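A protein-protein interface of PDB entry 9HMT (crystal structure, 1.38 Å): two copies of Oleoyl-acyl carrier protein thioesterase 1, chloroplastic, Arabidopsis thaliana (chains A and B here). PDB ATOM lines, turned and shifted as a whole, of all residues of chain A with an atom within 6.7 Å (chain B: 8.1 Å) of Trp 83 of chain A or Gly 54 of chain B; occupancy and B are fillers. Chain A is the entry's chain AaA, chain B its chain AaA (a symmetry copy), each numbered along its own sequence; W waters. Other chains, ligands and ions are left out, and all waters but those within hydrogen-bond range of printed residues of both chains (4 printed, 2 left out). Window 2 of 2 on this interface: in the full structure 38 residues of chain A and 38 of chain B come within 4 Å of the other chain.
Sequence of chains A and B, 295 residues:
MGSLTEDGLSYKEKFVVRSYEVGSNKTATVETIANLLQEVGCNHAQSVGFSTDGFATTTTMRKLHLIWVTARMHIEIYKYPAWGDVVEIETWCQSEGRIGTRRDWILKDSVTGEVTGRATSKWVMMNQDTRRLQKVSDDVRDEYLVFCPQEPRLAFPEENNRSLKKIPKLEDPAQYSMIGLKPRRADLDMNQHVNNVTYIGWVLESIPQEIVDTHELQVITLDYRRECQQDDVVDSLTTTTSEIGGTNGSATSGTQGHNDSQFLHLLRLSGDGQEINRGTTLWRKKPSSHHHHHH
CA of Arg 18 of chain A touches OE1 of Glu 39 of chain B, at 3.5 Å. Ser 19 of chain A touches Met 190 of chain B. CB of Tyr 20 of chain A touches OE1 of Gln 38 of chain B, at 3.6 Å. Met 190 of chain B touches Val 22 of chain A. Met 190 of chain B touches Lys 26 of chain A. Trp 83 of chain A touches Gln 46 of chain B. Thr 52 of chain B touches Trp 83 of chain A (O to CE3, 3.6 Å). Trp 83 of chain A touches Asp 53 of chain B (CZ3 to C, 3.6 Å). Trp 83 of chain A touches Gly 54 of chain B. Trp 83 of chain A touches Met 190 of chain B (CZ3 to CE, 3.6 Å).
OE1 of Gln 38 of chain B sits at hydrogen-bond distance from OG of Ser 19 of chain A, 3.0 Å away. The backbone carbonyl oxygen (O) of Asp 53 of chain B lies close to the side-chain amino group (NZ) of Lys 26 of chain A (3.3 Å). The backbone NH (N) of Ser 19 of chain A is in hydrogen-bond range of the side-chain carboxylate (OE1) of Glu 39 of chain B. SG of Cys 42 of chain B sits at hydrogen-bond distance from OG of Ser 19 of chain A.
Water W2 lies within hydrogen-bond range of OD1 of Asn 43 of chain B (2.7 Å), NE1 of Trp 83 of chain A (2.8 Å), OE1 of Glu 39 of chain B (2.9 Å) and NE2 of Gln 46 of chain B (3.4 Å). Water W4 lies within hydrogen-bond range of O of Trp 83 of chain A (2.8 Å) and O of Thr 52 of chain B (2.9 Å). Water W3 bridges O of Ser 19 of chain A and N of Met 190 of chain B. Water W1 lies within hydrogen-bond range of the side-chain amide nitrogen (NE2) of Gln 46 of chain B, the indole nitrogen (NE1) of Trp 83 of chain A and the side-chain amide oxygen (OD1) of Asn 43 of chain B.
No position is printed for both chains. Of the 14 pairs that touch across the chains among the printed residues, none has its exchanged pair printed and touching as well.
N of Asp 53 of chain B lies within hydrogen-bond range of OG of Ser 51 of chain B (3.0 Å). The side-chain carboxylate (OE2) of Glu 39 of chain B lies within hydrogen-bond range of the side-chain amide nitrogen (ND2) of Asn 43 of chain B, at 3.0 Å. The backbone NH (N) of Trp 83 of chain A is in hydrogen-bond range of the backbone carbonyl oxygen (O) of Lys 26 of chain A (3.0 Å). The backbone carbonyl oxygen (O) of Cys 42 of chain B is in hydrogen-bond range of the side-chain amide nitrogen (NE2) of Gln 46 of chain B (3.4 Å). NH1 of Arg 18 of chain A lies within hydrogen-bond range of OH of Tyr 20 of chain A, 2.8 Å away. The side-chain sulfur (SG) of Cys 42 of chain B is in hydrogen-bond range of the backbone carbonyl oxygen (O) of Gln 38 of chain B, 3.5 Å away.
Hydrophobic or aromatic side chains of chain B within 4 Å of the printed part of chain A: Met 190. Of the 15 printed residues of chain A, 6 touch a printed residue of chain B. Among the printed residues, 14 pairs touch across the chains. Among the printed residues, no Asp or Glu carboxylate lies within 4 Å of a Lys or Arg side-chain nitrogen of the other chain.
Printed residues of chain B within 4 Å of Tyr 20 of chain A: Gln 38. Of the printed residues of chain B, Trp 83 of chain A touches Gln 46, Thr 52, Asp 53, Gly 54 and Met 190. Of the printed residues of chain A, Gln 46 of chain B touches Trp 83 (3.6 Å). Of chain A, only Trp 83 (3.4 Å) comes within 4 Å of Gly 54 of chain B. The nearest printed residue of chain A that does not touch Gln 38 of chain B is Arg 18 of chain A (6.5 Å).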
ATOM      1  N   VAL A  16       0.589   7.683  13.306  1.00  0.00           N
ATOM      2  CA  VAL A  16      -0.372   6.871  14.097  1.00  0.00           C
ATOM      3  C   VAL A  16      -0.727   7.671  15.349  1.00  0.00           C
ATOM      4  O   VAL A  16       0.181   8.030  16.137  1.00  0.00           O
ATOM      5  CB  VAL A  16       0.241   5.507  14.435  1.00  0.00           C
ATOM      6  CG1 VAL A  16      -0.712   4.701  15.288  1.00  0.00           C
ATOM      7  CG2 VAL A  16       0.637   4.735  13.181  1.00  0.00           C
ATOM      8  N   VAL A  17      -1.992   8.004  15.518  1.00  0.00           N
ATOM      9  CA  VAL A  17      -2.411   8.872  16.648  1.00  0.00           C
ATOM     10  C   VAL A  17      -2.124   8.148  17.962  1.00  0.00           C
ATOM     11  O   VAL A  17      -2.577   6.996  18.120  1.00  0.00           O
ATOM     12  CB  VAL A  17      -3.889   9.252  16.521  1.00  0.00           C
ATOM     13  CG1 VAL A  17      -4.365  10.044  17.712  1.00  0.00           C
ATOM     14  CG2 VAL A  17      -4.150   9.989  15.215  1.00  0.00           C
ATOM     15  N   ARG A  18      -1.466   8.832  18.877  1.00  0.00           N
ATOM     16  CA  ARG A  18      -0.982   8.233  20.145  1.00  0.00           C
ATOM     17  C   ARG A  18      -2.032   8.402  21.250  1.00  0.00           C
ATOM     18  O   ARG A  18      -2.863   9.302  21.196  1.00  0.00           O
ATOM     19  CB  ARG A  18       0.337   8.886  20.525  1.00  0.00           C
ATOM     20  CG  ARG A  18       1.446   8.628  19.524  1.00  0.00           C
ATOM     21  CD  ARG A  18       2.718   9.338  19.876  1.00  0.00           C
ATOM     22  NE  ARG A  18       3.779   9.024  18.940  1.00  0.00           N
ATOM     23  CZ  ARG A  18       4.963   9.635  18.913  1.00  0.00           C
ATOM     24  NH1 ARG A  18       5.253  10.564  19.805  1.00  0.00           N
ATOM     25  NH2 ARG A  18       5.854   9.306  18.002  1.00  0.00           N
ATOM     26  N   SER A  19      -1.884   7.577  22.283  1.00  0.00           N
ATOM     27  CA  SER A  19      -2.788   7.538  23.455  1.00  0.00           C
ATOM     28  C   SER A  19      -2.906   8.926  24.076  1.00  0.00           C
ATOM     29  O   SER A  19      -4.042   9.378  24.357  1.00  0.00           O
ATOM     30  CB  SER A  19      -2.254   6.529  24.464  1.00  0.00           C
ATOM     31  OG  SER A  19      -0.960   6.848  24.886  1.00  0.00           O
ATOM     32  N   TYR A  20      -1.791   9.616  24.244  1.00  0.00           N
ATOM     33  CA  TYR A  20      -1.751  10.896  24.992  1.00  0.00           C
ATOM     34  C   TYR A  20      -2.120  12.069  24.076  1.00  0.00           C
ATOM     35  O   TYR A  20      -2.187  13.195  24.558  1.00  0.00           O
ATOM     36  CB  TYR A  20      -0.397  11.099  25.662  1.00  0.00           C
ATOM     37  CG  TYR A  20       0.773  11.134  24.724  1.00  0.00           C
ATOM     38  CD1 TYR A  20       1.150  12.327  24.112  1.00  0.00           C
ATOM     39  CD2 TYR A  20       1.557  10.019  24.481  1.00  0.00           C
ATOM     40  CE1 TYR A  20       2.255  12.393  23.291  1.00  0.00           C
ATOM     41  CE2 TYR A  20       2.676  10.075  23.664  1.00  0.00           C
ATOM     42  CZ  TYR A  20       3.017  11.269  23.046  1.00  0.00           C
ATOM     43  OH  TYR A  20       4.148  11.330  22.276  1.00  0.00           O
ATOM     44  N   VAL A  22      -4.981  12.268  22.374  1.00  0.00           N
ATOM     45  CA  VAL A  22      -6.453  12.320  22.214  1.00  0.00           C
ATOM     46  C   VAL A  22      -7.094  12.887  23.471  1.00  0.00           C
ATOM     47  O   VAL A  22      -6.541  12.739  24.573  1.00  0.00           O
ATOM     48  CB  VAL A  22      -7.053  10.963  21.820  1.00  0.00           C
ATOM     49  CG1 VAL A  22      -6.400  10.427  20.560  1.00  0.00           C
ATOM     50  CG2 VAL A  22      -6.996   9.955  22.942  1.00  0.00           C
ATOM     51  N   ASN A  25     -13.234  12.126  23.584  1.00  0.00           N
ATOM     52  CA  ASN A  25     -13.910  11.309  22.537  1.00  0.00           C
ATOM     53  C   ASN A  25     -12.903  10.362  21.879  1.00  0.00           C
ATOM     54  O   ASN A  25     -13.256   9.750  20.849  1.00  0.00           O
ATOM     55  CB  ASN A  25     -14.594  12.167  21.475  1.00  0.00           C
ATOM     56  CG  ASN A  25     -15.672  13.056  22.056  1.00  0.00           C
ATOM     57  OD1 ASN A  25     -15.541  14.277  22.046  1.00  0.00           O
ATOM     58  ND2 ASN A  25     -16.735  12.456  22.572  1.00  0.00           N
ATOM     59  N   LYS A  26     -11.697  10.270  22.445  1.00  0.00           N
ATOM     60  CA  LYS A  26     -10.622   9.370  21.972  1.00  0.00           C
ATOM     61  C   LYS A  26     -10.296   9.741  20.527  1.00  0.00           C
ATOM     62  O   LYS A  26      -9.863   8.866  19.773  1.00  0.00           O
ATOM     63  CB  LYS A  26     -11.017   7.894  22.099  1.00  0.00           C
ATOM     64  CG  LYS A  26     -11.092   7.393  23.534  1.00  0.00           C
ATOM     65  CD  LYS A  26     -12.243   6.455  23.798  1.00  0.00           C
ATOM     66  CE  LYS A  26     -12.833   6.593  25.189  1.00  0.00           C
ATOM     67  NZ  LYS A  26     -14.172   5.963  25.262  1.00  0.00           N
ATOM     68  N   THR A  27     -10.420  11.027  20.179  1.00  0.00           N
ATOM     69  CA  THR A  27      -9.901  11.515  18.893  1.00  0.00           C
ATOM     70  C   THR A  27      -8.836  12.575  19.174  1.00  0.00           C
ATOM     71  O   THR A  27      -8.834  13.213  20.239  1.00  0.00           O
ATOM     72  CB  THR A  27     -10.992  12.034  17.950  1.00  0.00           C
ATOM     73  OG1 THR A  27     -11.660  13.117  18.589  1.00  0.00           O
ATOM     74  CG2 THR A  27     -11.994  10.967  17.556  1.00  0.00           C
ATOM     75  N   ALA A  28      -7.958  12.732  18.197  1.00  0.00           N
ATOM     76  CA  ALA A  28      -6.846  13.691  18.285  1.00  0.00           C
ATOM     77  C   ALA A  28      -7.407  15.063  18.632  1.00  0.00           C
ATOM     78  O   ALA A  28      -8.412  15.495  18.027  1.00  0.00           O
ATOM     79  CB  ALA A  28      -6.074  13.752  16.992  1.00  0.00           C
ATOM     80  N   PRO A  81      -9.040  12.254  13.738  1.00  0.00           N
ATOM     81  CA  PRO A  81      -8.705  10.837  13.720  1.00  0.00           C
ATOM     82  C   PRO A  81      -8.701  10.238  15.120  1.00  0.00           C
ATOM     83  O   PRO A  81      -8.308  10.897  16.095  1.00  0.00           O
ATOM     84  CB  PRO A  81      -7.306  10.787  13.126  1.00  0.00           C
ATOM     85  CG  PRO A  81      -6.710  12.134  13.455  1.00  0.00           C
ATOM     86  CD  PRO A  81      -7.890  13.091  13.373  1.00  0.00           C
ATOM     87  N   ALA A  82      -9.109   8.976  15.213  1.00  0.00           N
ATOM     88  CA  ALA A  82      -9.161   8.287  16.510  1.00  0.00           C
ATOM     89  C   ALA A  82      -7.772   7.824  16.932  1.00  0.00           C
ATOM     90  O   ALA A  82      -6.878   7.627  16.130  1.00  0.00           O
ATOM     91  CB  ALA A  82     -10.114   7.116  16.452  1.00  0.00           C
ATOM     92  N   TRP A  83      -7.652   7.610  18.221  1.00  0.00           N
ATOM     93  CA  TRP A  83      -6.549   6.858  18.836  1.00  0.00           C
ATOM     94  C   TRP A  83      -6.233   5.601  18.009  1.00  0.00           C
ATOM     95  O   TRP A  83      -7.152   4.789  17.782  1.00  0.00           O
ATOM     96  CB  TRP A  83      -6.960   6.522  20.254  1.00  0.00           C
ATOM     97  CG  TRP A  83      -5.966   5.740  21.036  1.00  0.00           C
ATOM     98  CD1 TRP A  83      -4.632   5.594  20.829  1.00  0.00           C
ATOM     99  CD2 TRP A  83      -6.273   5.014  22.234  1.00  0.00           C
ATOM    100  NE1 TRP A  83      -4.077   4.835  21.827  1.00  0.00           N
ATOM    101  CE2 TRP A  83      -5.071   4.433  22.681  1.00  0.00           C
ATOM    102  CE3 TRP A  83      -7.457   4.774  22.947  1.00  0.00           C
ATOM    103  CZ2 TRP A  83      -4.999   3.653  23.835  1.00  0.00           C
ATOM    104  CZ3 TRP A  83      -7.386   3.989  24.078  1.00  0.00           C
ATOM    105  CH2 TRP A  83      -6.175   3.454  24.524  1.00  0.00           C
ATOM    106  N   GLY A  84      -5.000   5.478  17.541  1.00  0.00           N
ATOM    107  CA  GLY A  84      -4.526   4.317  16.771  1.00  0.00           C
ATOM    108  C   GLY A  84      -4.799   4.409  15.275  1.00  0.00           C
ATOM    109  O   GLY A  84      -4.267   3.565  14.544  1.00  0.00           O
ATOM    110  N   ASP A  85      -5.550   5.412  14.824  1.00  0.00           N
ATOM    111  CA  ASP A  85      -5.800   5.620  13.379  1.00  0.00           C
ATOM    112  C   ASP A  85      -4.527   6.175  12.751  1.00  0.00           C
ATOM    113  O   ASP A  85      -3.726   6.862  13.431  1.00  0.00           O
ATOM    114  CB  ASP A  85      -6.905   6.635  13.110  1.00  0.00           C
ATOM    115  CG  ASP A  85      -8.323   6.161  13.373  1.00  0.00           C
ATOM    116  OD1 ASP A  85      -8.485   4.964  13.705  1.00  0.00           O
ATOM    117  OD2 ASP A  85      -9.256   7.003  13.228  1.00  0.00           O
ATOM    118  N   GLN B  38       4.795   5.699  28.016  1.00  0.00           N
ATOM    119  CA  GLN B  38       3.334   5.500  28.146  1.00  0.00           C
ATOM    120  C   GLN B  38       2.772   4.910  26.853  1.00  0.00           C
ATOM    121  O   GLN B  38       1.953   3.987  26.901  1.00  0.00           O
ATOM    122  CB  GLN B  38       2.577   6.808  28.408  1.00  0.00           C
ATOM    123  CG  GLN B  38       1.076   6.579  28.525  1.00  0.00           C
ATOM    124  CD  GLN B  38       0.282   7.853  28.472  1.00  0.00           C
ATOM    125  OE1 GLN B  38      -0.581   8.038  27.602  1.00  0.00           O
ATOM    126  NE2 GLN B  38       0.585   8.731  29.414  1.00  0.00           N
ATOM    127  N   GLU B  39       3.147   5.478  25.707  1.00  0.00           N
ATOM    128  CA  GLU B  39       2.566   5.046  24.417  1.00  0.00           C
ATOM    129  C   GLU B  39       2.927   3.586  24.146  1.00  0.00           C
ATOM    130  O   GLU B  39       2.047   2.823  23.726  1.00  0.00           O
ATOM    131  CB  GLU B  39       3.012   5.997  23.312  1.00  0.00           C
ATOM    132  CG  GLU B  39       2.621   5.567  21.917  1.00  0.00           C
ATOM    133  CD  GLU B  39       1.148   5.507  21.578  1.00  0.00           C
ATOM    134  OE1 GLU B  39       0.329   5.876  22.433  1.00  0.00           O
ATOM    135  OE2 GLU B  39       0.829   5.160  20.401  1.00  0.00           O
ATOM    136  N   GLY B  41       3.629   1.291  26.287  1.00  0.00           N
ATOM    137  CA  GLY B  41       2.847   0.507  27.267  1.00  0.00           C
ATOM    138  C   GLY B  41       1.422   0.328  26.801  1.00  0.00           C
ATOM    139  O   GLY B  41       0.867  -0.797  26.845  1.00  0.00           O
ATOM    140  N   CYS B  42       0.784   1.402  26.327  1.00  0.00           N
ATOM    141  CA  CYS B  42      -0.589   1.321  25.809  1.00  0.00           C
ATOM    142  C   CYS B  42      -0.682   0.431  24.582  1.00  0.00           C
ATOM    143  O   CYS B  42      -1.673  -0.314  24.446  1.00  0.00           O
ATOM    144  CB  CYS B  42      -1.113   2.697  25.425  1.00  0.00           C
ATOM    145  SG  CYS B  42      -1.508   3.727  26.845  1.00  0.00           S
ATOM    146  N   ASN B  43       0.302   0.487  23.707  1.00  0.00           N
ATOM    147  CA  ASN B  43       0.278  -0.343  22.482  1.00  0.00           C
ATOM    148  C   ASN B  43       0.510  -1.802  22.870  1.00  0.00           C
ATOM    149  O   ASN B  43      -0.117  -2.677  22.273  1.00  0.00           O
ATOM    150  CB  ASN B  43       1.267   0.175  21.458  1.00  0.00           C
ATOM    151  CG  ASN B  43       0.763   1.457  20.833  1.00  0.00           C
ATOM    152  OD1 ASN B  43      -0.441   1.707  20.795  1.00  0.00           O
ATOM    153  ND2 ASN B  43       1.704   2.258  20.365  1.00  0.00           N
ATOM    154  N   ALA B  45      -0.492  -3.143  25.697  1.00  0.00           N
ATOM    155  CA  ALA B  45      -1.801  -3.544  26.259  1.00  0.00           C
ATOM    156  C   ALA B  45      -2.739  -3.890  25.114  1.00  0.00           C
ATOM    157  O   ALA B  45      -3.424  -4.923  25.169  1.00  0.00           O
ATOM    158  CB  ALA B  45      -2.364  -2.488  27.168  1.00  0.00           C
ATOM    159  N   GLN B  46      -2.820  -3.061  24.079  1.00  0.00           N
ATOM    160  CA  GLN B  46      -3.777  -3.363  22.995  1.00  0.00           C
ATOM    161  C   GLN B  46      -3.374  -4.643  22.292  1.00  0.00           C
ATOM    162  O   GLN B  46      -4.287  -5.411  21.856  1.00  0.00           O
ATOM    163  CB  GLN B  46      -3.822  -2.200  22.015  1.00  0.00           C
ATOM    164  CG  GLN B  46      -4.543  -1.051  22.651  1.00  0.00           C
ATOM    165  CD  GLN B  46      -4.591   0.153  21.754  1.00  0.00           C
ATOM    166  OE1 GLN B  46      -5.488   0.302  20.924  1.00  0.00           O
ATOM    167  NE2 GLN B  46      -3.594   1.003  21.901  1.00  0.00           N
ATOM    168  N   PHE B  50      -6.178  -6.028  25.376  1.00  0.00           N
ATOM    169  CA  PHE B  50      -6.861  -4.972  26.146  1.00  0.00           C
ATOM    170  C   PHE B  50      -7.510  -4.022  25.123  1.00  0.00           C
ATOM    171  O   PHE B  50      -7.270  -4.086  23.868  1.00  0.00           O
ATOM    172  CB  PHE B  50      -5.906  -4.267  27.114  1.00  0.00           C
ATOM    173  CG  PHE B  50      -5.437  -5.137  28.257  1.00  0.00           C
ATOM    174  CD1 PHE B  50      -6.201  -5.286  29.395  1.00  0.00           C
ATOM    175  CD2 PHE B  50      -4.246  -5.842  28.172  1.00  0.00           C
ATOM    176  CE1 PHE B  50      -5.772  -6.101  30.438  1.00  0.00           C
ATOM    177  CE2 PHE B  50      -3.812  -6.646  29.222  1.00  0.00           C
ATOM    178  CZ  PHE B  50      -4.574  -6.777  30.354  1.00  0.00           C
ATOM    179  N   SER B  51      -8.392  -3.198  25.639  1.00  0.00           N
ATOM    180  CA  SER B  51      -9.278  -2.298  24.854  1.00  0.00           C
ATOM    181  C   SER B  51      -8.494  -1.436  23.860  1.00  0.00           C
ATOM    182  O   SER B  51      -7.377  -0.931  24.193  1.00  0.00           O
ATOM    183  CB  SER B  51     -10.049  -1.421  25.772  1.00  0.00           C
ATOM    184  OG  SER B  51     -10.972  -0.630  25.019  1.00  0.00           O
ATOM    185  N   THR B  52      -9.107  -1.176  22.703  1.00  0.00           N
ATOM    186  CA  THR B  52      -8.589  -0.186  21.725  1.00  0.00           C
ATOM    187  C   THR B  52      -9.264   1.178  21.927  1.00  0.00           C
ATOM    188  O   THR B  52      -8.947   2.100  21.131  1.00  0.00           O
ATOM    189  CB  THR B  52      -8.706  -0.701  20.285  1.00  0.00           C
ATOM    190  OG1 THR B  52     -10.085  -0.936  19.992  1.00  0.00           O
ATOM    191  CG2 THR B  52      -7.880  -1.950  20.058  1.00  0.00           C
ATOM    192  N   ASP B  53     -10.131   1.350  22.933  1.00  0.00           N
ATOM    193  CA  ASP B  53     -10.710   2.698  23.210  1.00  0.00           C
ATOM    194  C   ASP B  53     -10.770   3.015  24.712  1.00  0.00           C
ATOM    195  O   ASP B  53     -11.497   3.957  25.078  1.00  0.00           O
ATOM    196  CB  ASP B  53     -12.070   2.872  22.529  1.00  0.00           C
ATOM    197  CG  ASP B  53     -13.072   1.798  22.893  1.00  0.00           C
ATOM    198  OD1 ASP B  53     -13.041   1.341  24.050  1.00  0.00           O
ATOM    199  OD2 ASP B  53     -13.863   1.418  22.009  1.00  0.00           O
ATOM    200  N   GLY B  54      -9.997   2.334  25.569  1.00  0.00           N
ATOM    201  CA  GLY B  54      -9.723   2.847  26.927  1.00  0.00           C
ATOM    202  C   GLY B  54      -8.406   2.315  27.451  1.00  0.00           C
ATOM    203  O   GLY B  54      -7.873   1.396  26.847  1.00  0.00           O
ATOM    204  N   PHE B  55      -7.911   2.839  28.566  1.00  0.00           N
ATOM    205  CA  PHE B  55      -6.701   2.277  29.215  1.00  0.00           C
ATOM    206  C   PHE B  55      -7.004   0.868  29.726  1.00  0.00           C
ATOM    207  O   PHE B  55      -8.161   0.550  30.054  1.00  0.00           O
ATOM    208  CB  PHE B  55      -6.210   3.172  30.345  1.00  0.00           C
ATOM    209  CG  PHE B  55      -5.718   4.519  29.892  1.00  0.00           C
ATOM    210  CD1 PHE B  55      -4.682   4.610  28.977  1.00  0.00           C
ATOM    211  CD2 PHE B  55      -6.245   5.683  30.425  1.00  0.00           C
ATOM    212  CE1 PHE B  55      -4.192   5.845  28.584  1.00  0.00           C
ATOM    213  CE2 PHE B  55      -5.760   6.918  30.022  1.00  0.00           C
ATOM    214  CZ  PHE B  55      -4.745   6.996  29.098  1.00  0.00           C
ATOM    215  N   ALA B  56      -5.965   0.040  29.727  1.00  0.00           N
ATOM    216  CA  ALA B  56      -6.050  -1.402  30.012  1.00  0.00           C
ATOM    217  C   ALA B  56      -6.775  -1.681  31.337  1.00  0.00           C
ATOM    218  O   ALA B  56      -6.444  -1.131  32.410  1.00  0.00           O
ATOM    219  CB  ALA B  56      -4.667  -1.997  29.997  1.00  0.00           C
ATOM    220  N   THR B  57      -7.791  -2.512  31.248  1.00  0.00           N
ATOM    221  CA  THR B  57      -8.429  -3.171  32.407  1.00  0.00           C
ATOM    222  C   THR B  57      -8.689  -4.618  32.057  1.00  0.00           C
ATOM    223  O   THR B  57      -9.007  -4.897  30.886  1.00  0.00           O
ATOM    224  CB  THR B  57      -9.763  -2.517  32.782  1.00  0.00           C
ATOM    225  OG1 THR B  57     -10.641  -2.556  31.650  1.00  0.00           O
ATOM    226  CG2 THR B  57      -9.561  -1.108  33.283  1.00  0.00           C
ATOM    227  N   MET B 190      -7.515  11.046  28.018  1.00  0.00           N
ATOM    228  CA  MET B 190      -8.811  10.750  27.350  1.00  0.00           C
ATOM    229  C   MET B 190      -9.941  10.591  28.380  1.00  0.00           C
ATOM    230  O   MET B 190     -11.119  10.601  27.953  1.00  0.00           O
ATOM    231  CB  MET B 190      -8.717   9.503  26.466  1.00  0.00           C
ATOM    232  CG  MET B 190      -8.520   8.199  27.223  1.00  0.00           C
ATOM    233  SD  MET B 190      -8.253   6.804  26.099  1.00  0.00           S
ATOM    234  CE  MET B 190      -6.558   7.104  25.585  1.00  0.00           C
ATOM    235  N   ASN B 191      -9.627  10.519  29.672  1.00  0.00           N
ATOM    236  CA  ASN B 191     -10.665  10.446  30.736  1.00  0.00           C
ATOM    237  C   ASN B 191     -10.735  11.740  31.541  1.00  0.00           C
ATOM    238  O   ASN B 191     -11.370  11.749  32.605  1.00  0.00           O
ATOM    239  CB  ASN B 191     -10.393   9.263  31.646  1.00  0.00           C
ATOM    240  CG  ASN B 191     -10.473   7.979  30.862  1.00  0.00           C
ATOM    241  OD1 ASN B 191     -11.412   7.766  30.089  1.00  0.00           O
ATOM    242  ND2 ASN B 191      -9.456   7.152  31.013  1.00  0.00           N
HETATM  243  O   HOH W   1      -3.516   2.615  19.446  1.00  0.00           O
HETATM  244  O   HOH W   2      -1.538   3.672  22.323  1.00  0.00           O
HETATM  245  O   HOH W   3      -5.001   9.985  26.927  1.00  0.00           O
HETATM  246  O   HOH W   4      -9.479   4.164  19.156  1.00  0.00           O
